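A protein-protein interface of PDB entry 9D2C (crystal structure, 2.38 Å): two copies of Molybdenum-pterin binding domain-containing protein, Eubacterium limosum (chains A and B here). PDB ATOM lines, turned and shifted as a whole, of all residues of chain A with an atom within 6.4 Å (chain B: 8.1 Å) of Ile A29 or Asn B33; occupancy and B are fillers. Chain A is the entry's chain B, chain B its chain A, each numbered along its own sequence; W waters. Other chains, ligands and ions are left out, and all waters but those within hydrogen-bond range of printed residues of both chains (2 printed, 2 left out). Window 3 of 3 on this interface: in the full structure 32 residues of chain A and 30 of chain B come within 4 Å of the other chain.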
ATOM      1  N   GLN A   8      -0.230 -20.717  22.229  1.00  0.00           N
ATOM      2  CA  GLN A   8       0.698 -20.098  23.191  1.00  0.00           C
ATOM      3  C   GLN A   8       1.740 -19.320  22.384  1.00  0.00           C
ATOM      4  O   GLN A   8       2.771 -19.852  21.976  1.00  0.00           O
ATOM      5  CB  GLN A   8       1.311 -21.172  24.085  1.00  0.00           C
ATOM      6  CG  GLN A   8       0.237 -21.806  24.979  1.00  0.00           C
ATOM      7  CD  GLN A   8       0.710 -22.969  25.835  1.00  0.00           C
ATOM      8  OE1 GLN A   8      -0.045 -23.924  26.052  1.00  0.00           O
ATOM      9  NE2 GLN A   8       1.937 -22.882  26.359  1.00  0.00           N
ATOM     10  N   LEU A   9       1.482 -18.037  22.177  1.00  0.00           N
ATOM     11  CA  LEU A   9       2.188 -17.264  21.158  1.00  0.00           C
ATOM     12  C   LEU A   9       3.096 -16.242  21.822  1.00  0.00           C
ATOM     13  O   LEU A   9       2.616 -15.294  22.451  1.00  0.00           O
ATOM     14  CB  LEU A   9       1.177 -16.588  20.234  1.00  0.00           C
ATOM     15  CG  LEU A   9       0.267 -17.553  19.457  1.00  0.00           C
ATOM     16  CD1 LEU A   9      -0.796 -16.789  18.686  1.00  0.00           C
ATOM     17  CD2 LEU A   9       1.057 -18.450  18.487  1.00  0.00           C
ATOM     18  N   ALA A  10       4.405 -16.434  21.655  1.00  0.00           N
ATOM     19  CA  ALA A  10       5.383 -15.552  22.271  1.00  0.00           C
ATOM     20  C   ALA A  10       5.325 -14.182  21.629  1.00  0.00           C
ATOM     21  O   ALA A  10       5.116 -14.055  20.418  1.00  0.00           O
ATOM     22  CB  ALA A  10       6.793 -16.119  22.123  1.00  0.00           C
ATOM     23  N   GLY A  11       5.525 -13.156  22.445  1.00  0.00           N
ATOM     24  CA  GLY A  11       5.492 -11.796  21.942  1.00  0.00           C
ATOM     25  C   GLY A  11       5.937 -10.842  23.023  1.00  0.00           C
ATOM     26  O   GLY A  11       6.188 -11.230  24.165  1.00  0.00           O
ATOM     27  N   LYS A  12       5.981  -9.572  22.652  1.00  0.00           N
ATOM     28  CA  LYS A  12       6.428  -8.509  23.539  1.00  0.00           C
ATOM     29  C   LYS A  12       5.299  -7.500  23.758  1.00  0.00           C
ATOM     30  O   LYS A  12       4.528  -7.200  22.841  1.00  0.00           O
ATOM     31  CB  LYS A  12       7.669  -7.847  22.958  1.00  0.00           C
ATOM     32  CG  LYS A  12       8.964  -8.652  23.123  1.00  0.00           C
ATOM     33  CD  LYS A  12      10.151  -7.810  22.598  1.00  0.00           C
ATOM     34  CE  LYS A  12      11.527  -8.499  22.782  1.00  0.00           C
ATOM     35  NZ  LYS A  12      12.152  -8.366  24.133  1.00  0.00           N
ATOM     36  N   LEU A  27       0.057  -7.508  22.583  1.00  0.00           N
ATOM     37  CA  LEU A  27       1.319  -8.194  22.347  1.00  0.00           C
ATOM     38  C   LEU A  27       1.666  -8.196  20.862  1.00  0.00           C
ATOM     39  O   LEU A  27       0.836  -8.588  20.037  1.00  0.00           O
ATOM     40  CB  LEU A  27       1.237  -9.631  22.849  1.00  0.00           C
ATOM     41  CG  LEU A  27       1.312  -9.900  24.349  1.00  0.00           C
ATOM     42  CD1 LEU A  27       1.277 -11.429  24.539  1.00  0.00           C
ATOM     43  CD2 LEU A  27       2.531  -9.288  24.974  1.00  0.00           C
ATOM     44  N   ASP A  28       2.890  -7.766  20.531  1.00  0.00           N
ATOM     45  CA  ASP A  28       3.469  -7.962  19.198  1.00  0.00           C
ATOM     46  C   ASP A  28       4.027  -9.381  19.160  1.00  0.00           C
ATOM     47  O   ASP A  28       4.945  -9.698  19.924  1.00  0.00           O
ATOM     48  CB  ASP A  28       4.566  -6.927  18.936  1.00  0.00           C
ATOM     49  CG  ASP A  28       5.151  -6.992  17.503  1.00  0.00           C
ATOM     50  OD1 ASP A  28       5.608  -8.071  17.048  1.00  0.00           O
ATOM     51  OD2 ASP A  28       5.146  -5.932  16.826  1.00  0.00           O
ATOM     52  N   ILE A  29       3.455 -10.247  18.313  1.00  0.00           N
ATOM     53  CA  ILE A  29       3.878 -11.645  18.219  1.00  0.00           C
ATOM     54  C   ILE A  29       4.650 -11.933  16.937  1.00  0.00           C
ATOM     55  O   ILE A  29       4.900 -13.104  16.616  1.00  0.00           O
ATOM     56  CB  ILE A  29       2.697 -12.623  18.339  1.00  0.00           C
ATOM     57  CG1 ILE A  29       1.656 -12.356  17.247  1.00  0.00           C
ATOM     58  CG2 ILE A  29       2.062 -12.508  19.688  1.00  0.00           C
ATOM     59  CD1 ILE A  29       0.742 -13.553  16.949  1.00  0.00           C
ATOM     60  N   GLY A  30       5.007 -10.914  16.175  1.00  0.00           N
ATOM     61  CA  GLY A  30       5.759 -11.131  14.962  1.00  0.00           C
ATOM     62  C   GLY A  30       4.862 -11.336  13.757  1.00  0.00           C
ATOM     63  O   GLY A  30       3.647 -11.520  13.856  1.00  0.00           O
ATOM     64  N   GLY A  31       5.490 -11.294  12.590  1.00  0.00           N
ATOM     65  CA  GLY A  31       4.758 -11.448  11.354  1.00  0.00           C
ATOM     66  C   GLY A  31       3.727 -10.378  11.087  1.00  0.00           C
ATOM     67  O   GLY A  31       2.775 -10.623  10.338  1.00  0.00           O
ATOM     68  N   GLY A  32       3.867  -9.199  11.688  1.00  0.00           N
ATOM     69  CA  GLY A  32       2.880  -8.152  11.488  1.00  0.00           C
ATOM     70  C   GLY A  32       1.581  -8.337  12.245  1.00  0.00           C
ATOM     71  O   GLY A  32       0.603  -7.643  11.945  1.00  0.00           O
ATOM     72  N   ASN A  33       1.535  -9.257  13.202  1.00  0.00           N
ATOM     73  CA  ASN A  33       0.336  -9.566  13.960  1.00  0.00           C
ATOM     74  C   ASN A  33       0.433  -9.062  15.399  1.00  0.00           C
ATOM     75  O   ASN A  33       1.499  -9.103  16.021  1.00  0.00           O
ATOM     76  CB  ASN A  33       0.104 -11.075  13.941  1.00  0.00           C
ATOM     77  CG  ASN A  33      -0.355 -11.569  12.587  1.00  0.00           C
ATOM     78  OD1 ASN A  33      -1.218 -10.964  11.947  1.00  0.00           O
ATOM     79  ND2 ASN A  33       0.234 -12.665  12.135  1.00  0.00           N
ATOM     80  N   GLN A  34      -0.681  -8.580  15.922  1.00  0.00           N
ATOM     81  CA  GLN A  34      -0.775  -8.195  17.320  1.00  0.00           C
ATOM     82  C   GLN A  34      -1.966  -8.923  17.908  1.00  0.00           C
ATOM     83  O   GLN A  34      -2.930  -9.209  17.200  1.00  0.00           O
ATOM     84  CB  GLN A  34      -0.961  -6.692  17.495  1.00  0.00           C
ATOM     85  CG  GLN A  34       0.177  -5.851  16.956  1.00  0.00           C
ATOM     86  CD  GLN A  34      -0.014  -4.396  17.290  1.00  0.00           C
ATOM     87  OE1 GLN A  34      -1.124  -3.972  17.607  1.00  0.00           O
ATOM     88  NE2 GLN A  34       1.065  -3.624  17.252  1.00  0.00           N
ATOM     89  N   ILE A  35      -1.885  -9.240  19.195  1.00  0.00           N
ATOM     90  CA  ILE A  35      -2.967  -9.900  19.922  1.00  0.00           C
ATOM     91  C   ILE A  35      -3.338  -9.032  21.108  1.00  0.00           C
ATOM     92  O   ILE A  35      -2.463  -8.602  21.865  1.00  0.00           O
ATOM     93  CB  ILE A  35      -2.584 -11.325  20.362  1.00  0.00           C
ATOM     94  CG1 ILE A  35      -2.320 -12.157  19.101  1.00  0.00           C
ATOM     95  CG2 ILE A  35      -3.695 -11.918  21.249  1.00  0.00           C
ATOM     96  CD1 ILE A  35      -1.953 -13.579  19.334  1.00  0.00           C
ATOM     97  N   ALA A  57       0.651 -14.867  24.594  1.00  0.00           N
ATOM     98  CA  ALA A  57      -0.801 -14.829  24.467  1.00  0.00           C
ATOM     99  C   ALA A  57      -1.301 -16.266  24.464  1.00  0.00           C
ATOM    100  O   ALA A  57      -0.929 -17.044  23.577  1.00  0.00           O
ATOM    101  CB  ALA A  57      -1.228 -14.126  23.181  1.00  0.00           C
ATOM    102  N   LEU B   9      -6.830 -12.326  12.681  1.00  0.00           N
ATOM    103  CA  LEU B   9      -5.483 -12.604  12.191  1.00  0.00           C
ATOM    104  C   LEU B   9      -5.519 -13.412  10.899  1.00  0.00           C
ATOM    105  O   LEU B   9      -5.861 -14.600  10.922  1.00  0.00           O
ATOM    106  CB  LEU B   9      -4.693 -13.358  13.260  1.00  0.00           C
ATOM    107  CG  LEU B   9      -4.404 -12.666  14.585  1.00  0.00           C
ATOM    108  CD1 LEU B   9      -3.711 -13.578  15.549  1.00  0.00           C
ATOM    109  CD2 LEU B   9      -3.502 -11.482  14.274  1.00  0.00           C
ATOM    110  N   ALA B  10      -5.069 -12.797   9.805  1.00  0.00           N
ATOM    111  CA  ALA B  10      -5.089 -13.454   8.503  1.00  0.00           C
ATOM    112  C   ALA B  10      -4.100 -14.619   8.451  1.00  0.00           C
ATOM    113  O   ALA B  10      -2.996 -14.542   8.986  1.00  0.00           O
ATOM    114  CB  ALA B  10      -4.759 -12.436   7.409  1.00  0.00           C
ATOM    115  N   GLY B  11      -4.485 -15.687   7.762  1.00  0.00           N
ATOM    116  CA  GLY B  11      -3.640 -16.865   7.680  1.00  0.00           C
ATOM    117  C   GLY B  11      -4.214 -17.834   6.672  1.00  0.00           C
ATOM    118  O   GLY B  11      -5.247 -17.582   6.053  1.00  0.00           O
ATOM    119  N   LYS B  12      -3.505 -18.929   6.468  1.00  0.00           N
ATOM    120  CA  LYS B  12      -3.931 -19.931   5.498  1.00  0.00           C
ATOM    121  C   LYS B  12      -4.043 -21.275   6.204  1.00  0.00           C
ATOM    122  O   LYS B  12      -3.248 -21.593   7.089  1.00  0.00           O
ATOM    123  CB  LYS B  12      -2.987 -19.891   4.291  1.00  0.00           C
ATOM    124  CG  LYS B  12      -3.373 -20.685   3.074  1.00  0.00           C
ATOM    125  CD  LYS B  12      -2.441 -20.282   1.896  1.00  0.00           C
ATOM    126  CE  LYS B  12      -2.832 -18.839   1.378  1.00  0.00           C
ATOM    127  NZ  LYS B  12      -2.072 -18.368   0.164  1.00  0.00           N
ATOM    128  N   VAL B  14      -3.682 -24.883   7.190  1.00  0.00           N
ATOM    129  CA  VAL B  14      -2.693 -25.923   6.936  1.00  0.00           C
ATOM    130  C   VAL B  14      -3.232 -27.314   7.244  1.00  0.00           C
ATOM    131  O   VAL B  14      -2.722 -28.292   6.673  1.00  0.00           O
ATOM    132  CB  VAL B  14      -1.382 -25.670   7.707  1.00  0.00           C
ATOM    133  CG1 VAL B  14      -1.083 -24.177   7.741  1.00  0.00           C
ATOM    134  CG2 VAL B  14      -1.437 -26.256   9.099  1.00  0.00           C
ATOM    135  N   VAL B  26      -6.296 -25.648  11.791  1.00  0.00           N
ATOM    136  CA  VAL B  26      -5.037 -24.976  12.092  1.00  0.00           C
ATOM    137  C   VAL B  26      -4.721 -23.967  10.998  1.00  0.00           C
ATOM    138  O   VAL B  26      -4.703 -24.315   9.811  1.00  0.00           O
ATOM    139  CB  VAL B  26      -3.881 -25.975  12.238  1.00  0.00           C
ATOM    140  CG1 VAL B  26      -2.619 -25.206  12.462  1.00  0.00           C
ATOM    141  CG2 VAL B  26      -4.147 -26.942  13.379  1.00  0.00           C
ATOM    142  N   LEU B  27      -4.398 -22.739  11.401  1.00  0.00           N
ATOM    143  CA  LEU B  27      -4.115 -21.637  10.489  1.00  0.00           C
ATOM    144  C   LEU B  27      -2.666 -21.211  10.671  1.00  0.00           C
ATOM    145  O   LEU B  27      -2.215 -21.020  11.799  1.00  0.00           O
ATOM    146  CB  LEU B  27      -5.025 -20.441  10.769  1.00  0.00           C
ATOM    147  CG  LEU B  27      -5.726 -19.719   9.631  1.00  0.00           C
ATOM    148  CD1 LEU B  27      -6.639 -20.704   8.971  1.00  0.00           C
ATOM    149  CD2 LEU B  27      -6.477 -18.540  10.186  1.00  0.00           C
ATOM    150  N   ASP B  28      -1.927 -21.123   9.577  1.00  0.00           N
ATOM    151  CA  ASP B  28      -0.618 -20.490   9.579  1.00  0.00           C
ATOM    152  C   ASP B  28      -0.843 -18.994   9.474  1.00  0.00           C
ATOM    153  O   ASP B  28      -1.427 -18.547   8.486  1.00  0.00           O
ATOM    154  CB  ASP B  28       0.203 -20.988   8.391  1.00  0.00           C
ATOM    155  CG  ASP B  28       1.587 -20.381   8.344  1.00  0.00           C
ATOM    156  OD1 ASP B  28       1.788 -19.275   8.895  1.00  0.00           O
ATOM    157  OD2 ASP B  28       2.487 -21.024   7.773  1.00  0.00           O
ATOM    158  N   ILE B  29      -0.438 -18.216  10.478  1.00  0.00           N
ATOM    159  CA  ILE B  29      -0.666 -16.773  10.441  1.00  0.00           C
ATOM    160  C   ILE B  29       0.616 -15.999  10.165  1.00  0.00           C
ATOM    161  O   ILE B  29       0.616 -14.758  10.210  1.00  0.00           O
ATOM    162  CB  ILE B  29      -1.317 -16.287  11.742  1.00  0.00           C
ATOM    163  CG1 ILE B  29      -0.432 -16.685  12.926  1.00  0.00           C
ATOM    164  CG2 ILE B  29      -2.698 -16.872  11.871  1.00  0.00           C
ATOM    165  CD1 ILE B  29      -0.666 -15.889  14.179  1.00  0.00           C
ATOM    166  N   GLY B  30       1.701 -16.688   9.844  1.00  0.00           N
ATOM    167  CA  GLY B  30       2.951 -16.024   9.568  1.00  0.00           C
ATOM    168  C   GLY B  30       3.816 -15.877  10.802  1.00  0.00           C
ATOM    169  O   GLY B  30       3.420 -16.169  11.936  1.00  0.00           O
ATOM    170  N   GLY B  31       5.054 -15.461  10.551  1.00  0.00           N
ATOM    171  CA  GLY B  31       5.992 -15.284  11.630  1.00  0.00           C
ATOM    172  C   GLY B  31       6.255 -16.551  12.388  1.00  0.00           C
ATOM    173  O   GLY B  31       6.596 -16.496  13.570  1.00  0.00           O
ATOM    174  N   GLY B  32       6.027 -17.701  11.765  1.00  0.00           N
ATOM    175  CA  GLY B  32       6.227 -18.972  12.425  1.00  0.00           C
ATOM    176  C   GLY B  32       5.151 -19.357  13.410  1.00  0.00           C
ATOM    177  O   GLY B  32       5.358 -20.294  14.186  1.00  0.00           O
ATOM    178  N   ASN B  33       4.018 -18.664  13.415  1.00  0.00           N
ATOM    179  CA  ASN B  33       2.937 -18.907  14.363  1.00  0.00           C
ATOM    180  C   ASN B  33       1.734 -19.566  13.699  1.00  0.00           C
ATOM    181  O   ASN B  33       1.378 -19.252  12.556  1.00  0.00           O
ATOM    182  CB  ASN B  33       2.509 -17.592  15.014  1.00  0.00           C
ATOM    183  CG  ASN B  33       3.515 -17.093  16.035  1.00  0.00           C
ATOM    184  OD1 ASN B  33       4.005 -17.856  16.881  1.00  0.00           O
ATOM    185  ND2 ASN B  33       3.857 -15.815  15.935  1.00  0.00           N
ATOM    186  N   GLN B  34       1.108 -20.473  14.429  1.00  0.00           N
ATOM    187  CA  GLN B  34      -0.120 -21.111  13.998  1.00  0.00           C
ATOM    188  C   GLN B  34      -1.168 -20.983  15.089  1.00  0.00           C
ATOM    189  O   GLN B  34      -0.847 -20.970  16.277  1.00  0.00           O
ATOM    190  CB  GLN B  34       0.106 -22.569  13.677  1.00  0.00           C
ATOM    191  CG  GLN B  34       1.077 -22.789  12.551  1.00  0.00           C
ATOM    192  CD  GLN B  34       1.139 -24.250  12.130  1.00  0.00           C
ATOM    193  OE1 GLN B  34       0.794 -25.150  12.903  1.00  0.00           O
ATOM    194  NE2 GLN B  34       1.559 -24.491  10.894  1.00  0.00           N
ATOM    195  N   ILE B  35      -2.425 -20.946  14.664  1.00  0.00           N
ATOM    196  CA  ILE B  35      -3.576 -20.822  15.545  1.00  0.00           C
ATOM    197  C   ILE B  35      -4.449 -22.043  15.350  1.00  0.00           C
ATOM    198  O   ILE B  35      -4.869 -22.320  14.221  1.00  0.00           O
ATOM    199  CB  ILE B  35      -4.381 -19.554  15.215  1.00  0.00           C
ATOM    200  CG1 ILE B  35      -3.547 -18.308  15.460  1.00  0.00           C
ATOM    201  CG2 ILE B  35      -5.682 -19.536  16.051  1.00  0.00           C
ATOM    202  CD1 ILE B  35      -3.429 -17.976  16.890  1.00  0.00           C
ATOM    203  N   SER B  36      -4.773 -22.740  16.441  1.00  0.00           N
ATOM    204  CA  SER B  36      -5.712 -23.855  16.397  1.00  0.00           C
ATOM    205  C   SER B  36      -7.088 -23.374  16.829  1.00  0.00           C
ATOM    206  O   SER B  36      -7.218 -22.640  17.813  1.00  0.00           O
ATOM    207  CB  SER B  36      -5.284 -25.022  17.282  1.00  0.00           C
ATOM    208  OG  SER B  36      -4.096 -25.566  16.768  1.00  0.00           O
HETATM  209  O   HOH W   1       1.716 -12.368   8.340  1.00  0.00           O
HETATM  210  O   HOH W   2       2.350 -13.859  13.821  1.00  0.00           O
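The backbone carbonyl oxygen (O) of Ile B29 lies within hydrogen-bond range of the side-chain amide nitrogen (ND2) of Asn A33, 2.9 Å away. ND2 of Asn B33 lies within hydrogen-bond range of O of Ile A29 (3.0 Å).
N of Ile B35 lies within hydrogen-bond range of O of Leu B27 (2.9 Å). N of Ala A57 is in hydrogen-bond range of O of Leu A9, at 2.9 Å.
OD1 of Asn B33 touches CD2 of Leu A9 (3.4 Å). Gln B34 touches Leu A9 (O to CD2, 3.9 Å). Leu A9 touches Ile B35 (CD1 to CD1, 3.4 Å). CD1 of Ile B29 touches CD1 of Ile A29, 3.9 Å away. Asn A33 touches Leu B9. Leu B9 touches Gln A34.
Ile A29 touches two residues of chain B. Of the printed residues of chain A, Asn B33 touches Leu A9 (3.4 Å) and Ile A29 (3.0 Å). Of the printed residues of chain B, Asn A33 touches Leu B9 (3.3 Å) and Ile B29 (2.9 Å). Of the printed residues of chain A, Ile B35 touches Leu A9 (3.4 Å). Of the printed residues of chain B, Leu A9 touches Asn B33 (3.4 Å), Gln B34 (3.9 Å) and Ile B35 (3.4 Å). Printed residues of chain A within 4 Å of Ile B29: Ile A29 (3.9 Å) and Asn A33 (2.9 Å). Of the printed residues of chain B, Gln A34 touches Leu B9 (3.7 Å). The nearest residue of chain B that does not touch Ile A29 is Leu B9 (4.7 Å). The nearest residue of chain A that does not touch Asn B33 is Gly A30 (4.8 Å). The nearest printed residue of chain A that does not touch Gln B34 is Gln A8 (6.0 Å).
Hydrophobic or aromatic side chains of chain B that line the printed part of chain A: Leu B9, Ile B29 and Ile B35. Hydrophobic or aromatic side chains of chain A within 4 Å of the printed part of chain B: Leu A9 and Ile A29.
Leu A9 touches Asn B33, and with the chains exchanged Asn A33 touches Leu B9. Leu A9 touches Ile B35, but with the chains exchanged Ile A35 does not touch Leu B9 (4.1 Å). Ile A29 touches its own counterpart, Ile B29. Ile A29 touches Asn B33, and with the chains exchanged Asn A33 touches Ile B29. Of the 8 pairs that touch across the chains among the printed residues, 7 have their exchanged pair printed and touching as well.
Water W2 lies within hydrogen-bond range of the backbone carbonyl oxygen (O) of Gly A30, the side-chain amide nitrogen (ND2) of Asn A33, the backbone carbonyl oxygen (O) of Gly B30 and the side-chain amide nitrogen (ND2) of Asn B33. Water W1 bridges O of Gly A31 (2.9 Å) and O of Ile B29 (3.2 Å).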
